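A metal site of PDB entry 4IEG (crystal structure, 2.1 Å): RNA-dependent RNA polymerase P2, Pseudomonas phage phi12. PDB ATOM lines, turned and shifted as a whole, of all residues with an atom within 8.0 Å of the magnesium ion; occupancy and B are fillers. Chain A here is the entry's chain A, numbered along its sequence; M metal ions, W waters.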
ATOM      1  N   PHE A 346      31.054   5.461   0.588  1.00  0.00           N
ATOM      2  CA  PHE A 346      30.114   4.856  -0.370  1.00  0.00           C
ATOM      3  C   PHE A 346      30.362   3.360  -0.436  1.00  0.00           C
ATOM      4  O   PHE A 346      31.440   2.909  -0.845  1.00  0.00           O
ATOM      5  CB  PHE A 346      30.278   5.468  -1.770  1.00  0.00           C
ATOM      6  CG  PHE A 346      29.371   4.868  -2.814  1.00  0.00           C
ATOM      7  CD1 PHE A 346      28.092   5.366  -3.007  1.00  0.00           C
ATOM      8  CD2 PHE A 346      29.804   3.804  -3.604  1.00  0.00           C
ATOM      9  CE1 PHE A 346      27.245   4.821  -3.963  1.00  0.00           C
ATOM     10  CE2 PHE A 346      28.963   3.258  -4.576  1.00  0.00           C
ATOM     11  CZ  PHE A 346      27.683   3.761  -4.745  1.00  0.00           C
ATOM     12  N   PHE A 347      29.357   2.587  -0.034  1.00  0.00           N
ATOM     13  CA  PHE A 347      29.417   1.139  -0.099  1.00  0.00           C
ATOM     14  C   PHE A 347      28.736   0.734  -1.392  1.00  0.00           C
ATOM     15  O   PHE A 347      27.521   0.849  -1.547  1.00  0.00           O
ATOM     16  CB  PHE A 347      28.740   0.510   1.114  1.00  0.00           C
ATOM     17  CG  PHE A 347      29.545   0.616   2.378  1.00  0.00           C
ATOM     18  CD1 PHE A 347      29.725   1.841   2.993  1.00  0.00           C
ATOM     19  CD2 PHE A 347      30.129  -0.490   2.956  1.00  0.00           C
ATOM     20  CE1 PHE A 347      30.477   1.957   4.157  1.00  0.00           C
ATOM     21  CE2 PHE A 347      30.874  -0.386   4.118  1.00  0.00           C
ATOM     22  CZ  PHE A 347      31.047   0.840   4.712  1.00  0.00           C
ATOM     23  N   GLY A 348      29.553   0.291  -2.345  1.00  0.00           N
ATOM     24  CA  GLY A 348      29.068  -0.043  -3.665  1.00  0.00           C
ATOM     25  C   GLY A 348      28.378  -1.394  -3.715  1.00  0.00           C
ATOM     26  O   GLY A 348      28.711  -2.302  -2.968  1.00  0.00           O
ATOM     27  N   ASP A 349      27.406  -1.485  -4.617  1.00  0.00           N
ATOM     28  CA  ASP A 349      26.679  -2.701  -4.890  1.00  0.00           C
ATOM     29  C   ASP A 349      26.659  -2.829  -6.406  1.00  0.00           C
ATOM     30  O   ASP A 349      26.205  -1.917  -7.094  1.00  0.00           O
ATOM     31  CB  ASP A 349      25.233  -2.550  -4.374  1.00  0.00           C
ATOM     32  CG  ASP A 349      24.469  -3.859  -4.362  1.00  0.00           C
ATOM     33  OD1 ASP A 349      24.977  -4.886  -4.885  1.00  0.00           O
ATOM     34  OD2 ASP A 349      23.343  -3.861  -3.812  1.00  0.00           O
ATOM     35  N   VAL A 350      27.179  -3.951  -6.915  1.00  0.00           N
ATOM     36  CA  VAL A 350      27.313  -4.189  -8.356  1.00  0.00           C
ATOM     37  C   VAL A 350      26.371  -5.310  -8.826  1.00  0.00           C
ATOM     38  O   VAL A 350      26.259  -6.349  -8.162  1.00  0.00           O
ATOM     39  CB  VAL A 350      28.766  -4.567  -8.725  1.00  0.00           C
ATOM     40  CG1 VAL A 350      28.937  -4.670 -10.244  1.00  0.00           C
ATOM     41  CG2 VAL A 350      29.748  -3.525  -8.151  1.00  0.00           C
ATOM     42  N   ASN A 467      37.172  -5.767  -2.000  1.00  0.00           N
ATOM     43  CA  ASN A 467      37.069  -7.225  -1.935  1.00  0.00           C
ATOM     44  C   ASN A 467      36.222  -7.675  -3.116  1.00  0.00           C
ATOM     45  O   ASN A 467      35.056  -8.004  -2.965  1.00  0.00           O
ATOM     46  CB  ASN A 467      36.464  -7.684  -0.609  1.00  0.00           C
ATOM     47  CG  ASN A 467      36.240  -9.195  -0.532  1.00  0.00           C
ATOM     48  OD1 ASN A 467      36.819  -9.982  -1.309  1.00  0.00           O
ATOM     49  ND2 ASN A 467      35.391  -9.622   0.404  1.00  0.00           N
ATOM     50  N   ASP A 469      33.808  -7.592  -6.078  1.00  0.00           N
ATOM     51  CA  ASP A 469      32.655  -6.751  -6.392  1.00  0.00           C
ATOM     52  C   ASP A 469      32.201  -5.917  -5.181  1.00  0.00           C
ATOM     53  O   ASP A 469      31.415  -4.981  -5.334  1.00  0.00           O
ATOM     54  CB  ASP A 469      31.492  -7.566  -6.994  1.00  0.00           C
ATOM     55  CG  ASP A 469      30.856  -8.537  -6.018  1.00  0.00           C
ATOM     56  OD1 ASP A 469      31.556  -9.113  -5.151  1.00  0.00           O
ATOM     57  OD2 ASP A 469      29.610  -8.738  -6.136  1.00  0.00           O
ATOM     58  N   ASP A 470      32.723  -6.253  -3.994  1.00  0.00           N
ATOM     59  CA  ASP A 470      32.415  -5.553  -2.728  1.00  0.00           C
ATOM     60  C   ASP A 470      33.483  -4.512  -2.462  1.00  0.00           C
ATOM     61  O   ASP A 470      34.668  -4.844  -2.396  1.00  0.00           O
ATOM     62  CB  ASP A 470      32.417  -6.571  -1.584  1.00  0.00           C
ATOM     63  CG  ASP A 470      31.616  -6.129  -0.372  1.00  0.00           C
ATOM     64  OD1 ASP A 470      30.956  -5.055  -0.378  1.00  0.00           O
ATOM     65  OD2 ASP A 470      31.640  -6.901   0.611  1.00  0.00           O
ATOM     66  N   GLU A 471      33.078  -3.263  -2.316  1.00  0.00           N
ATOM     67  CA  GLU A 471      34.034  -2.176  -2.106  1.00  0.00           C
ATOM     68  C   GLU A 471      33.492  -1.075  -1.203  1.00  0.00           C
ATOM     69  O   GLU A 471      32.279  -0.891  -1.077  1.00  0.00           O
ATOM     70  CB  GLU A 471      34.482  -1.556  -3.454  1.00  0.00           C
ATOM     71  CG  GLU A 471      33.357  -0.879  -4.264  1.00  0.00           C
ATOM     72  CD  GLU A 471      33.853  -0.035  -5.448  1.00  0.00           C
ATOM     73  OE1 GLU A 471      35.043   0.348  -5.475  1.00  0.00           O
ATOM     74  OE2 GLU A 471      33.039   0.249  -6.354  1.00  0.00           O
ATOM     75  N   ILE A 472      34.415  -0.372  -0.565  1.00  0.00           N
ATOM     76  CA  ILE A 472      34.111   0.876   0.132  1.00  0.00           C
ATOM     77  C   ILE A 472      34.899   1.976  -0.569  1.00  0.00           C
ATOM     78  O   ILE A 472      36.122   1.864  -0.713  1.00  0.00           O
ATOM     79  CB  ILE A 472      34.530   0.840   1.614  1.00  0.00           C
ATOM     80  CG1 ILE A 472      33.896  -0.330   2.356  1.00  0.00           C
ATOM     81  CG2 ILE A 472      34.145   2.137   2.309  1.00  0.00           C
ATOM     82  CD1 ILE A 472      34.482  -0.569   3.749  1.00  0.00           C
ATOM     83  N   GLY A 501      25.474   0.707  -7.692  1.00  0.00           N
ATOM     84  CA  GLY A 501      24.598   1.560  -6.882  1.00  0.00           C
ATOM     85  C   GLY A 501      24.929   1.412  -5.404  1.00  0.00           C
ATOM     86  O   GLY A 501      25.706   0.537  -5.021  1.00  0.00           O
ATOM     87  N   PRO A 502      24.342   2.289  -4.554  1.00  0.00           N
ATOM     88  CA  PRO A 502      24.622   2.192  -3.134  1.00  0.00           C
ATOM     89  C   PRO A 502      23.996   0.941  -2.521  1.00  0.00           C
ATOM     90  O   PRO A 502      22.936   0.490  -2.986  1.00  0.00           O
ATOM     91  CB  PRO A 502      24.013   3.472  -2.548  1.00  0.00           C
ATOM     92  CG  PRO A 502      23.321   4.179  -3.676  1.00  0.00           C
ATOM     93  CD  PRO A 502      23.266   3.253  -4.836  1.00  0.00           C
ATOM     94  N   GLU A 503      24.647   0.382  -1.506  1.00  0.00           N
ATOM     95  CA  GLU A 503      24.254  -0.907  -0.952  1.00  0.00           C
ATOM     96  C   GLU A 503      23.425  -0.721   0.315  1.00  0.00           C
ATOM     97  O   GLU A 503      23.940  -0.196   1.305  1.00  0.00           O
ATOM     98  CB  GLU A 503      25.490  -1.778  -0.662  1.00  0.00           C
ATOM     99  CG  GLU A 503      25.153  -3.239  -0.401  1.00  0.00           C
ATOM    100  CD  GLU A 503      26.333  -4.117  -0.020  1.00  0.00           C
ATOM    101  OE1 GLU A 503      27.460  -3.608   0.233  1.00  0.00           O
ATOM    102  OE2 GLU A 503      26.127  -5.351   0.047  1.00  0.00           O
ATOM    103  N   GLU A 504      22.160  -1.137   0.277  1.00  0.00           N
ATOM    104  CA  GLU A 504      21.293  -1.080   1.467  1.00  0.00           C
ATOM    105  C   GLU A 504      21.917  -1.889   2.598  1.00  0.00           C
ATOM    106  O   GLU A 504      22.102  -3.101   2.479  1.00  0.00           O
ATOM    107  CB  GLU A 504      19.866  -1.564   1.167  1.00  0.00           C
ATOM    108  CG  GLU A 504      18.942  -0.467   0.584  1.00  0.00           C
ATOM    109  CD  GLU A 504      17.441  -0.680   0.895  1.00  0.00           C
ATOM    110  OE1 GLU A 504      16.763  -1.424   0.165  1.00  0.00           O
ATOM    111  OE2 GLU A 504      16.942  -0.055   1.856  1.00  0.00           O
ATOM    112  N   GLY A 505      22.267  -1.207   3.687  1.00  0.00           N
ATOM    113  CA  GLY A 505      22.925  -1.814   4.836  1.00  0.00           C
ATOM    114  C   GLY A 505      24.412  -1.528   4.932  1.00  0.00           C
ATOM    115  O   GLY A 505      25.012  -1.736   5.994  1.00  0.00           O
ATOM    116  N   ALA A 506      25.009  -1.048   3.830  1.00  0.00           N
ATOM    117  CA  ALA A 506      26.421  -0.695   3.771  1.00  0.00           C
ATOM    118  C   ALA A 506      27.263  -1.854   4.281  1.00  0.00           C
ATOM    119  O   ALA A 506      27.926  -1.760   5.320  1.00  0.00           O
ATOM    120  CB  ALA A 506      26.693   0.564   4.568  1.00  0.00           C
ATOM    121  N   VAL A 507      27.227  -2.959   3.543  1.00  0.00           N
ATOM    122  CA  VAL A 507      27.879  -4.211   3.923  1.00  0.00           C
ATOM    123  C   VAL A 507      29.217  -4.322   3.199  1.00  0.00           C
ATOM    124  O   VAL A 507      29.306  -4.042   2.011  1.00  0.00           O
ATOM    125  CB  VAL A 507      27.001  -5.437   3.569  1.00  0.00           C
ATOM    126  CG1 VAL A 507      27.635  -6.722   4.092  1.00  0.00           C
ATOM    127  CG2 VAL A 507      25.581  -5.283   4.118  1.00  0.00           C
ATOM    128  N   PHE A 508      30.259  -4.700   3.910  1.00  0.00           N
ATOM    129  CA  PHE A 508      31.542  -5.003   3.264  1.00  0.00           C
ATOM    130  C   PHE A 508      32.144  -6.240   3.897  1.00  0.00           C
ATOM    131  O   PHE A 508      32.330  -6.286   5.093  1.00  0.00           O
ATOM    132  CB  PHE A 508      32.530  -3.841   3.379  1.00  0.00           C
ATOM    133  CG  PHE A 508      33.905  -4.167   2.868  1.00  0.00           C
ATOM    134  CD1 PHE A 508      34.158  -4.174   1.506  1.00  0.00           C
ATOM    135  CD2 PHE A 508      34.945  -4.449   3.736  1.00  0.00           C
ATOM    136  CE1 PHE A 508      35.427  -4.465   1.015  1.00  0.00           C
ATOM    137  CE2 PHE A 508      36.230  -4.745   3.264  1.00  0.00           C
ATOM    138  CZ  PHE A 508      36.462  -4.747   1.900  1.00  0.00           C
ATOM    139  N   SER A 509      32.445  -7.240   3.066  1.00  0.00           N
ATOM    140  CA  SER A 509      33.010  -8.505   3.531  1.00  0.00           C
ATOM    141  C   SER A 509      32.280  -9.102   4.748  1.00  0.00           C
ATOM    142  O   SER A 509      32.913  -9.485   5.737  1.00  0.00           O
ATOM    143  CB  SER A 509      34.500  -8.311   3.823  1.00  0.00           C
ATOM    144  OG  SER A 509      35.145  -7.872   2.648  1.00  0.00           O
ATOM    145  N   GLY A 510      30.958  -9.193   4.646  1.00  0.00           N
ATOM    146  CA  GLY A 510      30.137  -9.928   5.604  1.00  0.00           C
ATOM    147  C   GLY A 510      29.559  -9.132   6.757  1.00  0.00           C
ATOM    148  O   GLY A 510      28.728  -9.652   7.512  1.00  0.00           O
ATOM    149  N   SER A 511      29.999  -7.879   6.933  1.00  0.00           N
ATOM    150  CA  SER A 511      29.607  -7.074   8.095  1.00  0.00           C
ATOM    151  C   SER A 511      28.933  -5.776   7.680  1.00  0.00           C
ATOM    152  O   SER A 511      29.469  -5.035   6.854  1.00  0.00           O
ATOM    153  CB  SER A 511      30.822  -6.752   8.988  1.00  0.00           C
ATOM    154  OG  SER A 511      31.165  -7.839   9.844  1.00  0.00           O
ATOM    155  N   TYR A 513      28.154  -2.045   8.203  1.00  0.00           N
ATOM    156  CA  TYR A 513      28.847  -0.923   8.849  1.00  0.00           C
ATOM    157  C   TYR A 513      27.836   0.082   9.399  1.00  0.00           C
ATOM    158  O   TYR A 513      27.413   1.038   8.733  1.00  0.00           O
ATOM    159  CB  TYR A 513      29.889  -0.295   7.911  1.00  0.00           C
ATOM    160  CG  TYR A 513      31.166  -1.107   7.906  1.00  0.00           C
ATOM    161  CD1 TYR A 513      31.199  -2.366   7.304  1.00  0.00           C
ATOM    162  CD2 TYR A 513      32.325  -0.668   8.545  1.00  0.00           C
ATOM    163  CE1 TYR A 513      32.331  -3.141   7.305  1.00  0.00           C
ATOM    164  CE2 TYR A 513      33.475  -1.439   8.558  1.00  0.00           C
ATOM    165  CZ  TYR A 513      33.474  -2.680   7.931  1.00  0.00           C
ATOM    166  OH  TYR A 513      34.611  -3.480   7.915  1.00  0.00           O
HETATM  167 MG    MG M   1      29.135  -4.465  -0.107  1.00  0.00          MG
HETATM  168  O   HOH W   1      29.784  -2.493  -0.559  1.00  0.00           O
HETATM  169  O   HOH W   2      28.569  -6.279   0.228  1.00  0.00           O
HETATM  170  O   HOH W   3      28.594  -4.859  -2.064  1.00  0.00           O
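Water W2 bridges the side-chain carboxylate (OE2) of Glu 503 (2.6 Å) and the side-chain carboxylate (OD2) of Asp 470 (3.2 Å).
Water W3 bridges O of Gly 348 (2.7 Å) and OE2 of Glu 503 (3.3 Å).
Water W1 lies within hydrogen-bond range of the backbone carbonyl oxygen of Gly 348 and the backbone carbonyl oxygen of Glu 471.
Merely in contact with the magnesium ion: Gly 348 (3.6 Å).
Within 4 Å of the magnesium ion: Gly 348, Asp 470, Glu 503 and Val 507.
The backbone NH (N) of Glu 503 lies within hydrogen-bond range of the backbone carbonyl oxygen (O) of Phe 347.
The backbone NH (N) of Gly 348 is in hydrogen-bond range of the backbone carbonyl oxygen (O) of Glu 471, at 3.2 Å.
OD2 of Asp 470 is in hydrogen-bond range of N of Ser 509, 2.6 Å away.
The magnesium ion is bound by OE1 of Glu 503 (1.9 Å), water W2 (1.9 Å), OD1 of Asp 470 (1.9 Å), water W3 (2.1 Å), water W1 (2.1 Å) and O of Val 507 (2.2 Å).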
